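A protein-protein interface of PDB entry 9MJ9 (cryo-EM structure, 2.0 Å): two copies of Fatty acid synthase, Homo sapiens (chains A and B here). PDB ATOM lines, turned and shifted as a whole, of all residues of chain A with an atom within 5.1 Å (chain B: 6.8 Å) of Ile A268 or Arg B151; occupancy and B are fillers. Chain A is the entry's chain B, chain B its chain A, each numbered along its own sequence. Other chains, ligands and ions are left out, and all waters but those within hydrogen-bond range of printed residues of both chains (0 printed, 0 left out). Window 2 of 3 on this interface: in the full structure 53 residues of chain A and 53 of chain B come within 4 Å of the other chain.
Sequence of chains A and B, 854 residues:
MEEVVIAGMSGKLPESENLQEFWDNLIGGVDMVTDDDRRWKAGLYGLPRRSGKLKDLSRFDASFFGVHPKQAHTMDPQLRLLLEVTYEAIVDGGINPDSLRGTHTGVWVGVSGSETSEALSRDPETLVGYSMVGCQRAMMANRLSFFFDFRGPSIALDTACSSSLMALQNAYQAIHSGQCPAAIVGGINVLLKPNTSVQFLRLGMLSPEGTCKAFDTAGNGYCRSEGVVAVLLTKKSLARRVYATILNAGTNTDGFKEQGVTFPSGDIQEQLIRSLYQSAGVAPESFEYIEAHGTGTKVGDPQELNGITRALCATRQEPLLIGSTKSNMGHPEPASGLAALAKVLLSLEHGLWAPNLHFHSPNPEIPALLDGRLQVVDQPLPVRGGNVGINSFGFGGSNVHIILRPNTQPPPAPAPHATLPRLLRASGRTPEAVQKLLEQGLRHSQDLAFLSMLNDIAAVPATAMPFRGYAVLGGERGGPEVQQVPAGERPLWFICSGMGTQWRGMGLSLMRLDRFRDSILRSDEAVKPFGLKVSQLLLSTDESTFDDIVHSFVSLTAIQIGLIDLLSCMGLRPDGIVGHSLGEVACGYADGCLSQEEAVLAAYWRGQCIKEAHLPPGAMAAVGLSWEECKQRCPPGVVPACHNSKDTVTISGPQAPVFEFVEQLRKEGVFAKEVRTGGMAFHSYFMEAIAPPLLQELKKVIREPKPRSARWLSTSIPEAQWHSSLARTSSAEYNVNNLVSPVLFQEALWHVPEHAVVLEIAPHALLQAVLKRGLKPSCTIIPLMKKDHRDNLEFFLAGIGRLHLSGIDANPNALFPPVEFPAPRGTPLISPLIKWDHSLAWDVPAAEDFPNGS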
ATOM      1  N   THR A 251      -9.018  18.198  -7.830  1.00  0.00           N
ATOM      2  CA  THR A 251      -7.956  18.374  -6.851  1.00  0.00           C
ATOM      3  C   THR A 251      -8.110  19.711  -6.139  1.00  0.00           C
ATOM      4  O   THR A 251      -8.747  20.634  -6.651  1.00  0.00           O
ATOM      5  CB  THR A 251      -6.576  18.283  -7.512  1.00  0.00           C
ATOM      6  OG1 THR A 251      -5.562  18.546  -6.539  1.00  0.00           O
ATOM      7  CG2 THR A 251      -6.445  19.282  -8.634  1.00  0.00           C
ATOM      8  N   ASN A 252      -7.524  19.804  -4.946  1.00  0.00           N
ATOM      9  CA  ASN A 252      -7.363  21.077  -4.246  1.00  0.00           C
ATOM     10  C   ASN A 252      -6.168  20.958  -3.302  1.00  0.00           C
ATOM     11  O   ASN A 252      -5.426  19.972  -3.337  1.00  0.00           O
ATOM     12  CB  ASN A 252      -8.647  21.496  -3.516  1.00  0.00           C
ATOM     13  CG  ASN A 252      -9.134  20.481  -2.516  1.00  0.00           C
ATOM     14  OD1 ASN A 252      -8.606  19.386  -2.398  1.00  0.00           O
ATOM     15  ND2 ASN A 252     -10.176  20.844  -1.796  1.00  0.00           N
ATOM     16  N   THR A 253      -5.971  21.972  -2.463  1.00  0.00           N
ATOM     17  CA  THR A 253      -4.886  22.007  -1.492  1.00  0.00           C
ATOM     18  C   THR A 253      -5.430  22.539  -0.176  1.00  0.00           C
ATOM     19  O   THR A 253      -6.401  23.297  -0.158  1.00  0.00           O
ATOM     20  CB  THR A 253      -3.712  22.879  -1.989  1.00  0.00           C
ATOM     21  OG1 THR A 253      -3.509  22.641  -3.383  1.00  0.00           O
ATOM     22  CG2 THR A 253      -2.413  22.543  -1.283  1.00  0.00           C
ATOM     23  N   ASP A 254      -4.807  22.120   0.929  1.00  0.00           N
ATOM     24  CA  ASP A 254      -5.285  22.481   2.261  1.00  0.00           C
ATOM     25  C   ASP A 254      -5.139  23.971   2.540  1.00  0.00           C
ATOM     26  O   ASP A 254      -6.007  24.573   3.173  1.00  0.00           O
ATOM     27  CB  ASP A 254      -4.531  21.678   3.316  1.00  0.00           C
ATOM     28  CG  ASP A 254      -4.892  20.215   3.303  1.00  0.00           C
ATOM     29  OD1 ASP A 254      -5.990  19.880   2.827  1.00  0.00           O
ATOM     30  OD2 ASP A 254      -4.081  19.400   3.775  1.00  0.00           O
ATOM     31  N   GLY A 255      -4.050  24.579   2.082  1.00  0.00           N
ATOM     32  CA  GLY A 255      -3.803  25.969   2.405  1.00  0.00           C
ATOM     33  C   GLY A 255      -3.099  26.110   3.743  1.00  0.00           C
ATOM     34  O   GLY A 255      -2.299  25.269   4.140  1.00  0.00           O
ATOM     35  N   SER A 265      -5.849  17.909   6.989  1.00  0.00           N
ATOM     36  CA  SER A 265      -7.101  18.642   7.327  1.00  0.00           C
ATOM     37  C   SER A 265      -8.301  17.977   6.642  1.00  0.00           C
ATOM     38  O   SER A 265      -8.378  18.052   5.401  1.00  0.00           O
ATOM     39  CB  SER A 265      -7.008  20.092   6.944  1.00  0.00           C
ATOM     40  OG  SER A 265      -6.972  20.245   5.533  1.00  0.00           O
ATOM     41  N   GLY A 266      -9.207  17.365   7.412  1.00  0.00           N
ATOM     42  CA  GLY A 266     -10.317  16.670   6.794  1.00  0.00           C
ATOM     43  C   GLY A 266     -11.400  17.543   6.223  1.00  0.00           C
ATOM     44  O   GLY A 266     -12.218  17.061   5.434  1.00  0.00           O
ATOM     45  N   ASP A 267     -11.418  18.824   6.587  1.00  0.00           N
ATOM     46  CA  ASP A 267     -12.463  19.724   6.110  1.00  0.00           C
ATOM     47  C   ASP A 267     -12.301  20.036   4.629  1.00  0.00           C
ATOM     48  O   ASP A 267     -13.281  20.031   3.873  1.00  0.00           O
ATOM     49  CB  ASP A 267     -12.439  21.003   6.938  1.00  0.00           C
ATOM     50  CG  ASP A 267     -13.823  21.498   7.272  1.00  0.00           C
ATOM     51  OD1 ASP A 267     -14.712  21.419   6.399  1.00  0.00           O
ATOM     52  OD2 ASP A 267     -14.024  21.954   8.414  1.00  0.00           O
ATOM     53  N   ILE A 268     -11.065  20.288   4.192  1.00  0.00           N
ATOM     54  CA  ILE A 268     -10.803  20.564   2.784  1.00  0.00           C
ATOM     55  C   ILE A 268     -11.015  19.313   1.939  1.00  0.00           C
ATOM     56  O   ILE A 268     -11.499  19.392   0.802  1.00  0.00           O
ATOM     57  CB  ILE A 268      -9.386  21.142   2.628  1.00  0.00           C
ATOM     58  CG1 ILE A 268      -9.115  22.148   3.745  1.00  0.00           C
ATOM     59  CG2 ILE A 268      -9.207  21.794   1.282  1.00  0.00           C
ATOM     60  CD1 ILE A 268      -9.845  23.458   3.596  1.00  0.00           C
ATOM     61  N   GLN A 269     -10.676  18.142   2.486  1.00  0.00           N
ATOM     62  CA  GLN A 269     -10.938  16.880   1.793  1.00  0.00           C
ATOM     63  C   GLN A 269     -12.435  16.625   1.642  1.00  0.00           C
ATOM     64  O   GLN A 269     -12.891  16.159   0.585  1.00  0.00           O
ATOM     65  CB  GLN A 269     -10.270  15.730   2.543  1.00  0.00           C
ATOM     66  CG  GLN A 269      -8.766  15.859   2.660  1.00  0.00           C
ATOM     67  CD  GLN A 269      -8.199  15.048   3.800  1.00  0.00           C
ATOM     68  OE1 GLN A 269      -8.925  14.354   4.502  1.00  0.00           O
ATOM     69  NE2 GLN A 269      -6.892  15.125   3.985  1.00  0.00           N
ATOM     70  N   GLU A 270     -13.211  16.936   2.683  1.00  0.00           N
ATOM     71  CA  GLU A 270     -14.663  16.815   2.613  1.00  0.00           C
ATOM     72  C   GLU A 270     -15.247  17.762   1.570  1.00  0.00           C
ATOM     73  O   GLU A 270     -16.158  17.383   0.817  1.00  0.00           O
ATOM     74  CB  GLU A 270     -15.261  17.089   3.990  1.00  0.00           C
ATOM     75  CG  GLU A 270     -16.751  17.310   4.009  1.00  0.00           C
ATOM     76  CD  GLU A 270     -17.227  17.939   5.293  1.00  0.00           C
ATOM     77  OE1 GLU A 270     -16.448  17.963   6.266  1.00  0.00           O
ATOM     78  OE2 GLU A 270     -18.379  18.410   5.331  1.00  0.00           O
ATOM     79  N   GLN A 271     -14.711  18.987   1.494  1.00  0.00           N
ATOM     80  CA  GLN A 271     -15.147  19.938   0.473  1.00  0.00           C
ATOM     81  C   GLN A 271     -14.845  19.430  -0.931  1.00  0.00           C
ATOM     82  O   GLN A 271     -15.670  19.588  -1.837  1.00  0.00           O
ATOM     83  CB  GLN A 271     -14.473  21.286   0.685  1.00  0.00           C
ATOM     84  CG  GLN A 271     -14.988  22.071   1.861  1.00  0.00           C
ATOM     85  CD  GLN A 271     -14.205  23.344   2.072  1.00  0.00           C
ATOM     86  OE1 GLN A 271     -13.557  23.841   1.154  1.00  0.00           O
ATOM     87  NE2 GLN A 271     -14.251  23.874   3.285  1.00  0.00           N
ATOM     88  N   LEU A 272     -13.672  18.820  -1.123  1.00  0.00           N
ATOM     89  CA  LEU A 272     -13.305  18.279  -2.430  1.00  0.00           C
ATOM     90  C   LEU A 272     -14.238  17.155  -2.856  1.00  0.00           C
ATOM     91  O   LEU A 272     -14.710  17.133  -4.005  1.00  0.00           O
ATOM     92  CB  LEU A 272     -11.860  17.791  -2.408  1.00  0.00           C
ATOM     93  CG  LEU A 272     -11.353  17.054  -3.647  1.00  0.00           C
ATOM     94  CD1 LEU A 272     -11.252  17.993  -4.823  1.00  0.00           C
ATOM     95  CD2 LEU A 272     -10.013  16.428  -3.372  1.00  0.00           C
ATOM     96  N   ASN A 399      -4.671  17.332  -2.309  1.00  0.00           N
ATOM     97  CA  ASN A 399      -5.778  16.345  -2.180  1.00  0.00           C
ATOM     98  C   ASN A 399      -6.358  16.050  -3.567  1.00  0.00           C
ATOM     99  O   ASN A 399      -6.668  17.015  -4.293  1.00  0.00           O
ATOM    100  CB  ASN A 399      -6.849  16.837  -1.205  1.00  0.00           C
ATOM    101  CG  ASN A 399      -6.382  16.822   0.235  1.00  0.00           C
ATOM    102  OD1 ASN A 399      -5.463  16.083   0.584  1.00  0.00           O
ATOM    103  ND2 ASN A 399      -7.002  17.634   1.075  1.00  0.00           N
ATOM    104  N   LEU B 100      -6.505  37.121  -1.519  1.00  0.00           N
ATOM    105  CA  LEU B 100      -6.492  35.805  -2.141  1.00  0.00           C
ATOM    106  C   LEU B 100      -6.379  34.683  -1.117  1.00  0.00           C
ATOM    107  O   LEU B 100      -6.031  33.558  -1.481  1.00  0.00           O
ATOM    108  CB  LEU B 100      -5.346  35.707  -3.146  1.00  0.00           C
ATOM    109  CG  LEU B 100      -5.261  36.732  -4.271  1.00  0.00           C
ATOM    110  CD1 LEU B 100      -3.885  36.708  -4.889  1.00  0.00           C
ATOM    111  CD2 LEU B 100      -6.309  36.463  -5.319  1.00  0.00           C
ATOM    112  N   ARG B 101      -6.691  34.958   0.150  1.00  0.00           N
ATOM    113  CA  ARG B 101      -6.407  34.020   1.232  1.00  0.00           C
ATOM    114  C   ARG B 101      -7.336  32.815   1.275  1.00  0.00           C
ATOM    115  O   ARG B 101      -7.045  31.864   1.996  1.00  0.00           O
ATOM    116  CB  ARG B 101      -6.489  34.727   2.584  1.00  0.00           C
ATOM    117  CG  ARG B 101      -5.313  35.600   2.933  1.00  0.00           C
ATOM    118  CD  ARG B 101      -4.064  34.800   3.140  1.00  0.00           C
ATOM    119  NE  ARG B 101      -4.029  34.190   4.460  1.00  0.00           N
ATOM    120  CZ  ARG B 101      -2.937  33.694   5.024  1.00  0.00           C
ATOM    121  NH1 ARG B 101      -1.763  33.755   4.424  1.00  0.00           N
ATOM    122  NH2 ARG B 101      -3.030  33.117   6.217  1.00  0.00           N
ATOM    123  N   GLY B 102      -8.451  32.822   0.571  1.00  0.00           N
ATOM    124  CA  GLY B 102      -9.309  31.656   0.660  1.00  0.00           C
ATOM    125  C   GLY B 102      -9.691  31.118  -0.696  1.00  0.00           C
ATOM    126  O   GLY B 102     -10.453  30.162  -0.811  1.00  0.00           O
ATOM    127  N   THR B 103      -9.148  31.742  -1.728  1.00  0.00           N
ATOM    128  CA  THR B 103      -9.572  31.514  -3.093  1.00  0.00           C
ATOM    129  C   THR B 103      -8.946  30.238  -3.643  1.00  0.00           C
ATOM    130  O   THR B 103      -8.109  29.595  -3.012  1.00  0.00           O
ATOM    131  CB  THR B 103      -9.211  32.720  -3.944  1.00  0.00           C
ATOM    132  OG1 THR B 103      -7.876  33.116  -3.634  1.00  0.00           O
ATOM    133  CG2 THR B 103     -10.134  33.867  -3.628  1.00  0.00           C
ATOM    134  N   HIS B 104      -9.343  29.889  -4.863  1.00  0.00           N
ATOM    135  CA  HIS B 104      -8.937  28.654  -5.513  1.00  0.00           C
ATOM    136  C   HIS B 104      -7.776  28.861  -6.475  1.00  0.00           C
ATOM    137  O   HIS B 104      -7.741  28.248  -7.542  1.00  0.00           O
ATOM    138  CB  HIS B 104     -10.136  28.042  -6.238  1.00  0.00           C
ATOM    139  CG  HIS B 104     -10.080  26.552  -6.363  1.00  0.00           C
ATOM    140  ND1 HIS B 104      -9.522  25.918  -7.453  1.00  0.00           N
ATOM    141  CD2 HIS B 104     -10.507  25.572  -5.534  1.00  0.00           C
ATOM    142  CE1 HIS B 104      -9.616  24.611  -7.293  1.00  0.00           C
ATOM    143  NE2 HIS B 104     -10.206  24.376  -6.135  1.00  0.00           N
ATOM    144  N   THR B 105      -6.821  29.726  -6.135  1.00  0.00           N
ATOM    145  CA  THR B 105      -5.710  29.998  -7.033  1.00  0.00           C
ATOM    146  C   THR B 105      -4.660  28.900  -6.939  1.00  0.00           C
ATOM    147  O   THR B 105      -4.401  28.361  -5.863  1.00  0.00           O
ATOM    148  CB  THR B 105      -5.064  31.347  -6.726  1.00  0.00           C
ATOM    149  OG1 THR B 105      -4.092  31.190  -5.697  1.00  0.00           O
ATOM    150  CG2 THR B 105      -6.095  32.332  -6.267  1.00  0.00           C
ATOM    151  N   GLY B 106      -4.045  28.580  -8.074  1.00  0.00           N
ATOM    152  CA  GLY B 106      -3.099  27.494  -8.158  1.00  0.00           C
ATOM    153  C   GLY B 106      -1.648  27.928  -8.226  1.00  0.00           C
ATOM    154  O   GLY B 106      -1.336  29.081  -8.490  1.00  0.00           O
ATOM    155  N   SER B 145       1.795  27.412  -1.373  1.00  0.00           N
ATOM    156  CA  SER B 145       0.366  27.273  -1.109  1.00  0.00           C
ATOM    157  C   SER B 145       0.051  27.303   0.378  1.00  0.00           C
ATOM    158  O   SER B 145      -1.022  27.768   0.768  1.00  0.00           O
ATOM    159  CB  SER B 145      -0.165  25.983  -1.722  1.00  0.00           C
ATOM    160  OG  SER B 145      -0.057  26.004  -3.127  1.00  0.00           O
ATOM    161  N   ASP B 149      -1.958  30.628   1.638  1.00  0.00           N
ATOM    162  CA  ASP B 149      -3.291  30.051   1.842  1.00  0.00           C
ATOM    163  C   ASP B 149      -4.069  29.939   0.529  1.00  0.00           C
ATOM    164  O   ASP B 149      -5.129  30.531   0.345  1.00  0.00           O
ATOM    165  CB  ASP B 149      -4.077  30.832   2.899  1.00  0.00           C
ATOM    166  CG  ASP B 149      -5.155  30.006   3.550  1.00  0.00           C
ATOM    167  OD1 ASP B 149      -5.238  28.799   3.272  1.00  0.00           O
ATOM    168  OD2 ASP B 149      -5.938  30.566   4.343  1.00  0.00           O
ATOM    169  N   PHE B 150      -3.527  29.144  -0.382  1.00  0.00           N
ATOM    170  CA  PHE B 150      -4.100  28.937  -1.704  1.00  0.00           C
ATOM    171  C   PHE B 150      -4.748  27.563  -1.742  1.00  0.00           C
ATOM    172  O   PHE B 150      -4.144  26.581  -1.306  1.00  0.00           O
ATOM    173  CB  PHE B 150      -3.023  29.056  -2.778  1.00  0.00           C
ATOM    174  CG  PHE B 150      -2.555  30.456  -3.024  1.00  0.00           C
ATOM    175  CD1 PHE B 150      -3.315  31.543  -2.633  1.00  0.00           C
ATOM    176  CD2 PHE B 150      -1.350  30.681  -3.653  1.00  0.00           C
ATOM    177  CE1 PHE B 150      -2.876  32.827  -2.870  1.00  0.00           C
ATOM    178  CE2 PHE B 150      -0.911  31.958  -3.888  1.00  0.00           C
ATOM    179  CZ  PHE B 150      -1.677  33.034  -3.501  1.00  0.00           C
ATOM    180  N   ARG B 151      -5.968  27.490  -2.263  1.00  0.00           N
ATOM    181  CA  ARG B 151      -6.728  26.248  -2.283  1.00  0.00           C
ATOM    182  C   ARG B 151      -6.713  25.535  -3.627  1.00  0.00           C
ATOM    183  O   ARG B 151      -7.359  24.498  -3.755  1.00  0.00           O
ATOM    184  CB  ARG B 151      -8.181  26.512  -1.898  1.00  0.00           C
ATOM    185  CG  ARG B 151      -8.402  27.193  -0.570  1.00  0.00           C
ATOM    186  CD  ARG B 151      -7.911  26.363   0.585  1.00  0.00           C
ATOM    187  NE  ARG B 151      -7.892  27.116   1.834  1.00  0.00           N
ATOM    188  CZ  ARG B 151      -8.954  27.343   2.596  1.00  0.00           C
ATOM    189  NH1 ARG B 151     -10.157  26.919   2.252  1.00  0.00           N
ATOM    190  NH2 ARG B 151      -8.804  28.010   3.733  1.00  0.00           N
ATOM    191  N   GLY B 152      -6.024  26.058  -4.631  1.00  0.00           N
ATOM    192  CA  GLY B 152      -6.037  25.453  -5.943  1.00  0.00           C
ATOM    193  C   GLY B 152      -5.016  24.344  -6.074  1.00  0.00           C
ATOM    194  O   GLY B 152      -4.444  23.896  -5.084  1.00  0.00           O
ATOM    195  N   PRO B 153      -4.787  23.866  -7.295  1.00  0.00           N
ATOM    196  CA  PRO B 153      -3.763  22.833  -7.508  1.00  0.00           C
ATOM    197  C   PRO B 153      -2.365  23.352  -7.222  1.00  0.00           C
ATOM    198  O   PRO B 153      -2.039  24.505  -7.491  1.00  0.00           O
ATOM    199  CB  PRO B 153      -3.923  22.480  -8.990  1.00  0.00           C
ATOM    200  CG  PRO B 153      -5.252  22.997  -9.375  1.00  0.00           C
ATOM    201  CD  PRO B 153      -5.497  24.194  -8.538  1.00  0.00           C
ATOM    202  N   SER B 154      -1.526  22.478  -6.676  1.00  0.00           N
ATOM    203  CA  SER B 154      -0.175  22.849  -6.255  1.00  0.00           C
ATOM    204  C   SER B 154       0.798  21.803  -6.784  1.00  0.00           C
ATOM    205  O   SER B 154       1.012  20.772  -6.142  1.00  0.00           O
ATOM    206  CB  SER B 154      -0.102  22.970  -4.741  1.00  0.00           C
ATOM    207  OG  SER B 154       1.117  23.543  -4.330  1.00  0.00           O
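The side-chain hydroxyl of Ser B154 is in hydrogen-bond range of the side-chain hydroxyl of Ser B145 (3.0 Å).
The side-chain carboxylate (OD1) of Asp A254 lies within hydrogen-bond range of the side-chain hydroxyl (OG) of Ser A265 (2.9 Å).
The backbone carbonyl oxygen (O) of Ser B145 sits at hydrogen-bond distance from the backbone NH (N) of Phe B150, at 3.1 Å.
The backbone carbonyl oxygen (O) of Ile A268 lies within hydrogen-bond range of the side-chain amide nitrogen (ND2) of Asn A252 (3.3 Å).
The backbone carbonyl oxygen (O) of Thr B103 lies within hydrogen-bond range of the backbone NH (N) of Arg B151 (3.1 Å).
The guanidinium group (NE) of Arg B151 lies within salt-bridge range of the side-chain carboxylate (OD1) of Asp B149.
Ile A268 touches just one residue of chain B: Arg B151 (3.7 Å).
Of the printed residues of chain A, Ser B145 touches Gly A255.
Of the printed residues of chain A, Pro B153 touches Thr A251.
The nearest printed residue of chain A that does not touch Ser B154 is Thr A251 (5.6 Å).
The backbone NH (N) of Thr A253 lies within hydrogen-bond range of the backbone carbonyl oxygen (O) of Arg B151.
The side-chain hydroxyl (OG1) of Thr A253 sits close to the backbone carbonyl oxygen (O) of Gly B152 (2.3 Å).
The backbone carbonyl oxygen of Asp A254 lies within hydrogen-bond range of the guanidinium group of Arg B151, at 3.4 Å.
No position is printed for both chains.
CG2 of Thr A251 touches CG of Pro B153, 3.97 Å away.
CB of Asn A252 touches O of Arg B151, 3.3 Å away.
Asn A252 touches Gly B152 (C to O, 3.8 Å).
O of Phe B150 touches CB of Thr A253, at 3.8 Å.
Thr A253 touches Ser B154 (OG1 to CB, 3.7 Å).
Ser B145 touches Gly A255.
Gly A255 touches Asp B149 (CA to OD1, 3.3 Å).
Gly A255 touches Phe B150 (CA to O, 3.8 Å).
NH1 of Arg B151 touches CD1 of Ile A268, at 3.7 Å.
Of the 14 printed residues of chain A, 6 touch a printed residue of chain B.
Printed residues of chain A that touch a printed residue of chain B: Thr A251, Asn A252, Thr A253, Asp A254, Gly A255 and Ile A268.
Of the 14 printed residues of chain B, 7 touch a printed residue of chain A.
Hydrophobic or aromatic side chains of chain B that line the printed part of chain A: Pro B153.
Along chain B the printed residues that touch a printed residue of chain A span positions 145 to 154.
Among the printed residues, 12 pairs touch across the chains.
Among the printed residues, no Asp or Glu carboxylate lies within 4 Å of a Lys or Arg side-chain nitrogen of the other chain.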
